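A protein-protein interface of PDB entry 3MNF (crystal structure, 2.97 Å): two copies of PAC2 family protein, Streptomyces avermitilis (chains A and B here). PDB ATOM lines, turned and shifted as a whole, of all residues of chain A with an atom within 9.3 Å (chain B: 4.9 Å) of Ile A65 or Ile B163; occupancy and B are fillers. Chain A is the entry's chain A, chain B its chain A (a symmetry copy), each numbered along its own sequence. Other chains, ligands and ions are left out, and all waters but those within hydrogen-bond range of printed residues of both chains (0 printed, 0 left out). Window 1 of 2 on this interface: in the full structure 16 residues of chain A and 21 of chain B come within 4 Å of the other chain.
Of the printed residues of chain B, Phe A49 touches Trp B97. Of the printed residues of chain B, Pro A54 touches Trp B97 (3.6 Å) and Thr B158 (3.0 Å). Printed residues of chain B within 4 Å of Arg A63: Gly B162 (3.6 Å), Gln B165 (2.8 Å) and Glu B166 (3.2 Å). Lys A64 touches none of the printed residues of chain B. Ile A65 touches just these residues of chain B: Ile B163 (3.8 Å) and Glu B166 (3.4 Å). Of the printed residues of chain A, Trp B97 touches Glu A44 (3.7 Å), Phe A49 (3.5 Å) and Pro A54 (3.6 Å). Gly B159 touches none of the printed residues of chain A. Of chain A, only Arg A63 (3.6 Å) comes within 4 Å of Gly B162. Of the printed residues of chain A, Gln B165 touches Arg A63. The nearest residue of chain A that does not touch Ile B163 is Pro A54 (4.3 Å). The nearest printed residue of chain A that does not touch Trp B97 is Trp A67 (4.1 Å).
Of the 12 printed residues of chain B, 6 touch a printed residue of chain A. Hydrophobic or aromatic side chains of chain B that line the printed part of chain A: Trp B97 and Ile B163. Of the 19 printed residues of chain A, 7 touch a printed residue of chain B. Hydrophobic or aromatic side chains of chain A within 4 Å of the printed part of chain B: Phe A49, Pro A54, Ile A65 and Trp A67.
Glu A44 touches Trp B97 (OE1 to N, 3.7 Å). Phe A49 touches Trp B97 (CB to CE2, 3.5 Å). Pro A54 touches Trp B97. O of Gly B162 touches NH2 of Arg A63, at 3.6 Å. Ile A65 touches Ile B163 (CG1 to CD1, 3.8 Å). CD1 of Ile A65 touches CG of Glu B166 (3.4 Å). Trp A67 touches Ile B163 (CH2 to CD1, 3.9 Å).
The backbone carbonyl oxygen (O) of Trp B97 lies within hydrogen-bond range of the side-chain sulfur (SG) of Cys B101 (3.4 Å). The side-chain amide nitrogen (NE2) of Gln B165 lies within hydrogen-bond range of the side-chain carboxylate (OE2) of Glu B166.
The backbone carbonyl oxygen (O) of Thr B158 sits close to the guanidinium group (NE) of Arg A53 (3.3 Å). O of Pro A54 lies within hydrogen-bond range of N of Thr B158 (3.0 Å). NH2 of Arg A63 sits at hydrogen-bond distance from OE1 of Gln B165, 2.8 Å away. NE of Arg A63 lies within salt-bridge range of OE2 of Glu B166 (3.2 Å).
No position is printed for both chains. Of the 11 pairs that touch across the chains among the printed residues, none has its exchanged pair printed and touching as well.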
ATOM      1  N   GLU A  44      14.296  27.849 -23.586  1.00  0.00           N
ATOM      2  CA  GLU A  44      14.322  29.277 -23.285  1.00  0.00           C
ATOM      3  C   GLU A  44      13.010  29.837 -22.720  1.00  0.00           C
ATOM      4  O   GLU A  44      13.032  30.738 -21.890  1.00  0.00           O
ATOM      5  CB  GLU A  44      14.692  30.026 -24.538  1.00  0.00           C
ATOM      6  CG  GLU A  44      15.272  31.397 -24.334  1.00  0.00           C
ATOM      7  CD  GLU A  44      16.752  31.398 -23.994  1.00  0.00           C
ATOM      8  OE1 GLU A  44      17.286  30.370 -23.500  1.00  0.00           O
ATOM      9  OE2 GLU A  44      17.371  32.459 -24.201  1.00  0.00           O
ATOM     10  N   PHE A  49      17.091  27.807 -15.347  1.00  0.00           N
ATOM     11  CA  PHE A  49      18.256  26.988 -15.586  1.00  0.00           C
ATOM     12  C   PHE A  49      19.122  26.869 -14.360  1.00  0.00           C
ATOM     13  O   PHE A  49      20.153  26.204 -14.376  1.00  0.00           O
ATOM     14  CB  PHE A  49      19.061  27.502 -16.774  1.00  0.00           C
ATOM     15  CG  PHE A  49      18.317  27.461 -18.060  1.00  0.00           C
ATOM     16  CD1 PHE A  49      17.895  26.258 -18.594  1.00  0.00           C
ATOM     17  CD2 PHE A  49      18.044  28.618 -18.751  1.00  0.00           C
ATOM     18  CE1 PHE A  49      17.202  26.219 -19.797  1.00  0.00           C
ATOM     19  CE2 PHE A  49      17.341  28.590 -19.950  1.00  0.00           C
ATOM     20  CZ  PHE A  49      16.919  27.393 -20.470  1.00  0.00           C
ATOM     21  N   ASN A  52      17.254  23.799 -13.300  1.00  0.00           N
ATOM     22  CA  ASN A  52      17.500  22.749 -14.277  1.00  0.00           C
ATOM     23  C   ASN A  52      18.755  23.022 -15.047  1.00  0.00           C
ATOM     24  O   ASN A  52      18.709  23.392 -16.213  1.00  0.00           O
ATOM     25  CB  ASN A  52      16.349  22.665 -15.266  1.00  0.00           C
ATOM     26  CG  ASN A  52      15.066  22.226 -14.617  1.00  0.00           C
ATOM     27  OD1 ASN A  52      14.970  21.098 -14.136  1.00  0.00           O
ATOM     28  ND2 ASN A  52      14.060  23.113 -14.607  1.00  0.00           N
ATOM     29  N   ARG A  53      19.882  22.844 -14.385  1.00  0.00           N
ATOM     30  CA  ARG A  53      21.171  23.163 -14.948  1.00  0.00           C
ATOM     31  C   ARG A  53      21.445  22.320 -16.197  1.00  0.00           C
ATOM     32  O   ARG A  53      21.379  21.102 -16.136  1.00  0.00           O
ATOM     33  CB  ARG A  53      22.207  22.910 -13.874  1.00  0.00           C
ATOM     34  CG  ARG A  53      23.274  23.903 -13.896  1.00  0.00           C
ATOM     35  CD  ARG A  53      23.912  24.201 -12.553  1.00  0.00           C
ATOM     36  NE  ARG A  53      24.372  25.577 -12.637  1.00  0.00           N
ATOM     37  CZ  ARG A  53      23.953  26.537 -11.836  1.00  0.00           C
ATOM     38  NH1 ARG A  53      24.369  27.768 -12.016  1.00  0.00           N
ATOM     39  NH2 ARG A  53      23.133  26.258 -10.835  1.00  0.00           N
ATOM     40  N   PRO A  54      21.738  22.963 -17.345  1.00  0.00           N
ATOM     41  CA  PRO A  54      22.106  22.227 -18.555  1.00  0.00           C
ATOM     42  C   PRO A  54      23.455  21.534 -18.391  1.00  0.00           C
ATOM     43  O   PRO A  54      24.246  21.924 -17.535  1.00  0.00           O
ATOM     44  CB  PRO A  54      22.195  23.330 -19.607  1.00  0.00           C
ATOM     45  CG  PRO A  54      22.590  24.519 -18.878  1.00  0.00           C
ATOM     46  CD  PRO A  54      21.910  24.416 -17.525  1.00  0.00           C
ATOM     47  N   THR A  55      23.742  20.514 -19.180  1.00  0.00           N
ATOM     48  CA  THR A  55      25.021  19.798 -18.958  1.00  0.00           C
ATOM     49  C   THR A  55      25.979  19.838 -20.160  1.00  0.00           C
ATOM     50  O   THR A  55      25.574  20.085 -21.302  1.00  0.00           O
ATOM     51  CB  THR A  55      24.809  18.332 -18.469  1.00  0.00           C
ATOM     52  OG1 THR A  55      24.019  17.632 -19.432  1.00  0.00           O
ATOM     53  CG2 THR A  55      24.073  18.297 -17.115  1.00  0.00           C
ATOM     54  N   VAL A  56      27.253  19.621 -19.899  1.00  0.00           N
ATOM     55  CA  VAL A  56      28.213  19.581 -20.980  1.00  0.00           C
ATOM     56  C   VAL A  56      28.742  18.162 -21.147  1.00  0.00           C
ATOM     57  O   VAL A  56      29.100  17.512 -20.169  1.00  0.00           O
ATOM     58  CB  VAL A  56      29.358  20.626 -20.780  1.00  0.00           C
ATOM     59  CG1 VAL A  56      29.946  20.538 -19.400  1.00  0.00           C
ATOM     60  CG2 VAL A  56      30.438  20.473 -21.830  1.00  0.00           C
ATOM     61  N   TRP A  57      28.761  17.674 -22.380  1.00  0.00           N
ATOM     62  CA  TRP A  57      29.392  16.385 -22.681  1.00  0.00           C
ATOM     63  C   TRP A  57      30.397  16.485 -23.812  1.00  0.00           C
ATOM     64  O   TRP A  57      30.407  17.463 -24.567  1.00  0.00           O
ATOM     65  CB  TRP A  57      28.360  15.294 -22.976  1.00  0.00           C
ATOM     66  CG  TRP A  57      27.467  15.567 -24.148  1.00  0.00           C
ATOM     67  CD1 TRP A  57      26.426  16.465 -24.211  1.00  0.00           C
ATOM     68  CD2 TRP A  57      27.498  14.901 -25.414  1.00  0.00           C
ATOM     69  NE1 TRP A  57      25.829  16.412 -25.448  1.00  0.00           N
ATOM     70  CE2 TRP A  57      26.461  15.460 -26.206  1.00  0.00           C
ATOM     71  CE3 TRP A  57      28.309  13.887 -25.966  1.00  0.00           C
ATOM     72  CZ2 TRP A  57      26.211  15.038 -27.526  1.00  0.00           C
ATOM     73  CZ3 TRP A  57      28.059  13.464 -27.280  1.00  0.00           C
ATOM     74  CH2 TRP A  57      27.019  14.047 -28.045  1.00  0.00           C
ATOM     75  N   LEU A  58      31.248  15.468 -23.910  1.00  0.00           N
ATOM     76  CA  LEU A  58      32.309  15.439 -24.889  1.00  0.00           C
ATOM     77  C   LEU A  58      31.956  14.476 -26.000  1.00  0.00           C
ATOM     78  O   LEU A  58      31.698  13.296 -25.747  1.00  0.00           O
ATOM     79  CB  LEU A  58      33.608  15.040 -24.220  1.00  0.00           C
ATOM     80  CG  LEU A  58      34.107  16.096 -23.237  1.00  0.00           C
ATOM     81  CD1 LEU A  58      35.249  15.568 -22.354  1.00  0.00           C
ATOM     82  CD2 LEU A  58      34.513  17.364 -23.971  1.00  0.00           C
ATOM     83  N   ASP A  59      31.924  14.993 -27.225  1.00  0.00           N
ATOM     84  CA  ASP A  59      31.638  14.198 -28.419  1.00  0.00           C
ATOM     85  C   ASP A  59      32.867  14.178 -29.320  1.00  0.00           C
ATOM     86  O   ASP A  59      33.254  15.214 -29.873  1.00  0.00           O
ATOM     87  CB  ASP A  59      30.437  14.776 -29.173  1.00  0.00           C
ATOM     88  CG  ASP A  59      29.899  13.831 -30.246  1.00  0.00           C
ATOM     89  OD1 ASP A  59      30.426  12.708 -30.430  1.00  0.00           O
ATOM     90  OD2 ASP A  59      28.924  14.219 -30.907  1.00  0.00           O
ATOM     91  N   VAL A  62      35.093  17.166 -28.693  1.00  0.00           N
ATOM     92  CA  VAL A  62      34.442  18.476 -28.603  1.00  0.00           C
ATOM     93  C   VAL A  62      33.333  18.620 -27.537  1.00  0.00           C
ATOM     94  O   VAL A  62      32.483  17.740 -27.373  1.00  0.00           O
ATOM     95  CB  VAL A  62      33.884  18.878 -29.997  1.00  0.00           C
ATOM     96  CG1 VAL A  62      33.175  20.252 -29.960  1.00  0.00           C
ATOM     97  CG2 VAL A  62      34.988  18.868 -31.033  1.00  0.00           C
ATOM     98  N   ARG A  63      33.339  19.752 -26.832  1.00  0.00           N
ATOM     99  CA  ARG A  63      32.302  20.065 -25.852  1.00  0.00           C
ATOM    100  C   ARG A  63      30.939  20.332 -26.514  1.00  0.00           C
ATOM    101  O   ARG A  63      30.853  21.063 -27.512  1.00  0.00           O
ATOM    102  CB  ARG A  63      32.734  21.264 -24.993  1.00  0.00           C
ATOM    103  CG  ARG A  63      33.532  20.893 -23.756  1.00  0.00           C
ATOM    104  CD  ARG A  63      34.237  22.087 -23.121  1.00  0.00           C
ATOM    105  NE  ARG A  63      33.378  23.261 -23.002  1.00  0.00           N
ATOM    106  CZ  ARG A  63      32.777  23.659 -21.880  1.00  0.00           C
ATOM    107  NH1 ARG A  63      32.937  22.996 -20.740  1.00  0.00           N
ATOM    108  NH2 ARG A  63      32.000  24.738 -21.900  1.00  0.00           N
ATOM    109  N   LYS A  64      29.885  19.738 -25.948  1.00  0.00           N
ATOM    110  CA  LYS A  64      28.515  19.942 -26.430  1.00  0.00           C
ATOM    111  C   LYS A  64      27.502  20.080 -25.296  1.00  0.00           C
ATOM    112  O   LYS A  64      27.709  19.543 -24.221  1.00  0.00           O
ATOM    113  CB  LYS A  64      28.136  18.839 -27.410  1.00  0.00           C
ATOM    114  CG  LYS A  64      28.539  19.233 -28.814  1.00  0.00           C
ATOM    115  CD  LYS A  64      28.614  18.087 -29.783  1.00  0.00           C
ATOM    116  CE  LYS A  64      29.054  18.625 -31.136  1.00  0.00           C
ATOM    117  NZ  LYS A  64      28.193  18.094 -32.244  1.00  0.00           N
ATOM    118  N   ILE A  65      26.412  20.803 -25.523  1.00  0.00           N
ATOM    119  CA  ILE A  65      25.549  21.180 -24.419  1.00  0.00           C
ATOM    120  C   ILE A  65      24.173  20.561 -24.529  1.00  0.00           C
ATOM    121  O   ILE A  65      23.545  20.634 -25.567  1.00  0.00           O
ATOM    122  CB  ILE A  65      25.427  22.732 -24.294  1.00  0.00           C
ATOM    123  CG1 ILE A  65      26.673  23.309 -23.638  1.00  0.00           C
ATOM    124  CG2 ILE A  65      24.201  23.158 -23.486  1.00  0.00           C
ATOM    125  CD1 ILE A  65      27.568  23.961 -24.587  1.00  0.00           C
ATOM    126  N   THR A  66      23.692  19.971 -23.446  1.00  0.00           N
ATOM    127  CA  THR A  66      22.338  19.452 -23.417  1.00  0.00           C
ATOM    128  C   THR A  66      21.476  20.333 -22.514  1.00  0.00           C
ATOM    129  O   THR A  66      21.826  20.567 -21.361  1.00  0.00           O
ATOM    130  CB  THR A  66      22.337  18.002 -22.926  1.00  0.00           C
ATOM    131  OG1 THR A  66      23.287  17.245 -23.699  1.00  0.00           O
ATOM    132  CG2 THR A  66      20.954  17.376 -23.051  1.00  0.00           C
ATOM    133  N   TRP A  67      20.368  20.834 -23.048  1.00  0.00           N
ATOM    134  CA  TRP A  67      19.454  21.666 -22.276  1.00  0.00           C
ATOM    135  C   TRP A  67      18.337  20.806 -21.725  1.00  0.00           C
ATOM    136  O   TRP A  67      18.001  19.795 -22.325  1.00  0.00           O
ATOM    137  CB  TRP A  67      18.866  22.787 -23.160  1.00  0.00           C
ATOM    138  CG  TRP A  67      19.913  23.716 -23.667  1.00  0.00           C
ATOM    139  CD1 TRP A  67      20.635  23.578 -24.812  1.00  0.00           C
ATOM    140  CD2 TRP A  67      20.404  24.903 -23.021  1.00  0.00           C
ATOM    141  NE1 TRP A  67      21.543  24.606 -24.931  1.00  0.00           N
ATOM    142  CE2 TRP A  67      21.422  25.436 -23.848  1.00  0.00           C
ATOM    143  CE3 TRP A  67      20.075  25.574 -21.832  1.00  0.00           C
ATOM    144  CZ2 TRP A  67      22.108  26.610 -23.530  1.00  0.00           C
ATOM    145  CZ3 TRP A  67      20.757  26.731 -21.513  1.00  0.00           C
ATOM    146  CH2 TRP A  67      21.767  27.239 -22.364  1.00  0.00           C
ATOM    147  N   PRO A  68      17.741  21.200 -20.591  1.00  0.00           N
ATOM    148  CA  PRO A  68      16.495  20.563 -20.220  1.00  0.00           C
ATOM    149  C   PRO A  68      15.458  20.883 -21.270  1.00  0.00           C
ATOM    150  O   PRO A  68      15.402  22.013 -21.730  1.00  0.00           O
ATOM    151  CB  PRO A  68      16.115  21.270 -18.925  1.00  0.00           C
ATOM    152  CG  PRO A  68      16.906  22.519 -18.897  1.00  0.00           C
ATOM    153  CD  PRO A  68      18.160  22.207 -19.607  1.00  0.00           C
ATOM    154  N   THR A  69      14.649  19.912 -21.681  1.00  0.00           N
ATOM    155  CA  THR A  69      13.538  20.248 -22.577  1.00  0.00           C
ATOM    156  C   THR A  69      12.460  19.177 -22.641  1.00  0.00           C
ATOM    157  O   THR A  69      12.433  18.305 -21.811  1.00  0.00           O
ATOM    158  CB  THR A  69      14.035  20.725 -23.984  1.00  0.00           C
ATOM    159  OG1 THR A  69      12.963  21.410 -24.661  1.00  0.00           O
ATOM    160  CG2 THR A  69      14.592  19.557 -24.813  1.00  0.00           C
ATOM    161  N   ARG A  71      10.821  16.747 -25.514  1.00  0.00           N
ATOM    162  CA  ARG A  71      11.132  16.357 -26.867  1.00  0.00           C
ATOM    163  C   ARG A  71      10.042  15.448 -27.411  1.00  0.00           C
ATOM    164  O   ARG A  71       9.488  14.632 -26.676  1.00  0.00           O
ATOM    165  CB  ARG A  71      12.496  15.703 -26.904  1.00  0.00           C
ATOM    166  CG  ARG A  71      13.097  15.570 -28.292  1.00  0.00           C
ATOM    167  CD  ARG A  71      14.611  15.258 -28.230  1.00  0.00           C
ATOM    168  NE  ARG A  71      15.258  15.871 -27.059  1.00  0.00           N
ATOM    169  CZ  ARG A  71      16.050  16.941 -27.095  1.00  0.00           C
ATOM    170  NH1 ARG A  71      16.330  17.553 -28.256  1.00  0.00           N
ATOM    171  NH2 ARG A  71      16.575  17.393 -25.955  1.00  0.00           N
ATOM    172  N   TRP B  97      19.139  32.002 -20.746  1.00  0.00           N
ATOM    173  CA  TRP B  97      20.595  32.067 -20.937  1.00  0.00           C
ATOM    174  C   TRP B  97      21.038  32.267 -22.385  1.00  0.00           C
ATOM    175  O   TRP B  97      22.030  32.947 -22.623  1.00  0.00           O
ATOM    176  CB  TRP B  97      21.256  30.816 -20.399  1.00  0.00           C
ATOM    177  CG  TRP B  97      21.209  30.697 -18.916  1.00  0.00           C
ATOM    178  CD1 TRP B  97      20.497  31.473 -18.030  1.00  0.00           C
ATOM    179  CD2 TRP B  97      21.856  29.696 -18.135  1.00  0.00           C
ATOM    180  NE1 TRP B  97      20.684  31.019 -16.753  1.00  0.00           N
ATOM    181  CE2 TRP B  97      21.513  29.930 -16.789  1.00  0.00           C
ATOM    182  CE3 TRP B  97      22.706  28.629 -18.445  1.00  0.00           C
ATOM    183  CZ2 TRP B  97      22.002  29.143 -15.753  1.00  0.00           C
ATOM    184  CZ3 TRP B  97      23.164  27.834 -17.429  1.00  0.00           C
ATOM    185  CH2 TRP B  97      22.814  28.091 -16.093  1.00  0.00           C
ATOM    186  N   CYS B 101      23.255  35.488 -23.436  1.00  0.00           N
ATOM    187  CA  CYS B 101      24.542  35.352 -24.067  1.00  0.00           C
ATOM    188  C   CYS B 101      24.591  36.061 -25.384  1.00  0.00           C
ATOM    189  O   CYS B 101      25.615  36.662 -25.703  1.00  0.00           O
ATOM    190  CB  CYS B 101      24.884  33.899 -24.240  1.00  0.00           C
ATOM    191  SG  CYS B 101      25.379  33.211 -22.676  1.00  0.00           S
ATOM    192  N   THR B 158      26.821  22.519 -16.101  1.00  0.00           N
ATOM    193  CA  THR B 158      27.601  23.686 -16.439  1.00  0.00           C
ATOM    194  C   THR B 158      26.863  24.929 -15.977  1.00  0.00           C
ATOM    195  O   THR B 158      25.732  24.842 -15.542  1.00  0.00           O
ATOM    196  CB  THR B 158      27.888  23.720 -17.955  1.00  0.00           C
ATOM    197  OG1 THR B 158      28.962  24.625 -18.224  1.00  0.00           O
ATOM    198  CG2 THR B 158      26.665  24.121 -18.768  1.00  0.00           C
ATOM    199  N   GLY B 159      27.496  26.088 -16.058  1.00  0.00           N
ATOM    200  CA  GLY B 159      26.824  27.329 -15.689  1.00  0.00           C
ATOM    201  C   GLY B 159      26.837  28.332 -16.819  1.00  0.00           C
ATOM    202  O   GLY B 159      27.089  27.977 -17.974  1.00  0.00           O
ATOM    203  N   ILE B 160      26.561  29.591 -16.494  1.00  0.00           N
ATOM    204  CA  ILE B 160      26.512  30.624 -17.520  1.00  0.00           C
ATOM    205  C   ILE B 160      27.900  30.875 -18.112  1.00  0.00           C
ATOM    206  O   ILE B 160      27.998  31.316 -19.261  1.00  0.00           O
ATOM    207  CB  ILE B 160      25.885  31.950 -17.011  1.00  0.00           C
ATOM    208  CG1 ILE B 160      25.486  32.846 -18.178  1.00  0.00           C
ATOM    209  CG2 ILE B 160      26.862  32.716 -16.123  1.00  0.00           C
ATOM    210  CD1 ILE B 160      24.597  32.210 -19.186  1.00  0.00           C
ATOM    211  N   VAL B 161      28.957  30.612 -17.331  1.00  0.00           N
ATOM    212  CA  VAL B 161      30.335  30.773 -17.809  1.00  0.00           C
ATOM    213  C   VAL B 161      30.537  29.763 -18.916  1.00  0.00           C
ATOM    214  O   VAL B 161      30.938  30.109 -20.017  1.00  0.00           O
ATOM    215  CB  VAL B 161      31.392  30.517 -16.694  1.00  0.00           C
ATOM    216  CG1 VAL B 161      32.783  30.397 -17.280  1.00  0.00           C
ATOM    217  CG2 VAL B 161      31.353  31.599 -15.646  1.00  0.00           C
ATOM    218  N   GLY B 162      30.226  28.508 -18.619  1.00  0.00           N
ATOM    219  CA  GLY B 162      30.343  27.446 -19.615  1.00  0.00           C
ATOM    220  C   GLY B 162      29.544  27.783 -20.854  1.00  0.00           C
ATOM    221  O   GLY B 162      30.065  27.726 -21.972  1.00  0.00           O
ATOM    222  N   ILE B 163      28.276  28.142 -20.648  1.00  0.00           N
ATOM    223  CA  ILE B 163      27.389  28.484 -21.747  1.00  0.00           C
ATOM    224  C   ILE B 163      27.924  29.641 -22.575  1.00  0.00           C
ATOM    225  O   ILE B 163      27.923  29.574 -23.787  1.00  0.00           O
ATOM    226  CB  ILE B 163      25.953  28.775 -21.249  1.00  0.00           C
ATOM    227  CG1 ILE B 163      25.303  27.498 -20.694  1.00  0.00           C
ATOM    228  CG2 ILE B 163      25.088  29.342 -22.357  1.00  0.00           C
ATOM    229  CD1 ILE B 163      25.466  26.261 -21.552  1.00  0.00           C
ATOM    230  N   LEU B 164      28.394  30.689 -21.910  1.00  0.00           N
ATOM    231  CA  LEU B 164      28.853  31.887 -22.594  1.00  0.00           C
ATOM    232  C   LEU B 164      30.080  31.574 -23.437  1.00  0.00           C
ATOM    233  O   LEU B 164      30.164  31.962 -24.611  1.00  0.00           O
ATOM    234  CB  LEU B 164      29.148  33.029 -21.608  1.00  0.00           C
ATOM    235  CG  LEU B 164      29.801  34.268 -22.253  1.00  0.00           C
ATOM    236  CD1 LEU B 164      28.937  34.926 -23.336  1.00  0.00           C
ATOM    237  CD2 LEU B 164      30.218  35.285 -21.192  1.00  0.00           C
ATOM    238  N   GLN B 165      31.027  30.857 -22.840  1.00  0.00           N
ATOM    239  CA  GLN B 165      32.236  30.479 -23.548  1.00  0.00           C
ATOM    240  C   GLN B 165      31.865  29.617 -24.763  1.00  0.00           C
ATOM    241  O   GLN B 165      32.462  29.755 -25.820  1.00  0.00           O
ATOM    242  CB  GLN B 165      33.234  29.830 -22.607  1.00  0.00           C
ATOM    243  CG  GLN B 165      34.368  29.143 -23.286  1.00  0.00           C
ATOM    244  CD  GLN B 165      34.053  27.686 -23.539  1.00  0.00           C
ATOM    245  OE1 GLN B 165      33.559  26.999 -22.650  1.00  0.00           O
ATOM    246  NE2 GLN B 165      34.331  27.203 -24.755  1.00  0.00           N
ATOM    247  N   GLU B 166      30.835  28.791 -24.657  1.00  0.00           N
ATOM    248  CA  GLU B 166      30.413  28.024 -25.834  1.00  0.00           C
ATOM    249  C   GLU B 166      29.659  28.835 -26.887  1.00  0.00           C
ATOM    250  O   GLU B 166      29.815  28.590 -28.082  1.00  0.00           O
ATOM    251  CB  GLU B 166      29.648  26.763 -25.446  1.00  0.00           C
ATOM    252  CG  GLU B 166      30.552  25.653 -24.932  1.00  0.00           C
ATOM    253  CD  GLU B 166      31.544  25.154 -25.986  1.00  0.00           C
ATOM    254  OE1 GLU B 166      31.119  24.952 -27.151  1.00  0.00           O
ATOM    255  OE2 GLU B 166      32.746  24.971 -25.643  1.00  0.00           O
ATOM    256  N   ALA B 167      28.853  29.797 -26.436  1.00  0.00           N
ATOM    257  CA  ALA B 167      28.132  30.688 -27.327  1.00  0.00           C
ATOM    258  C   ALA B 167      29.126  31.469 -28.178  1.00  0.00           C
ATOM    259  O   ALA B 167      28.903  31.662 -29.378  1.00  0.00           O
ATOM    260  CB  ALA B 167      27.247  31.629 -26.539  1.00  0.00           C
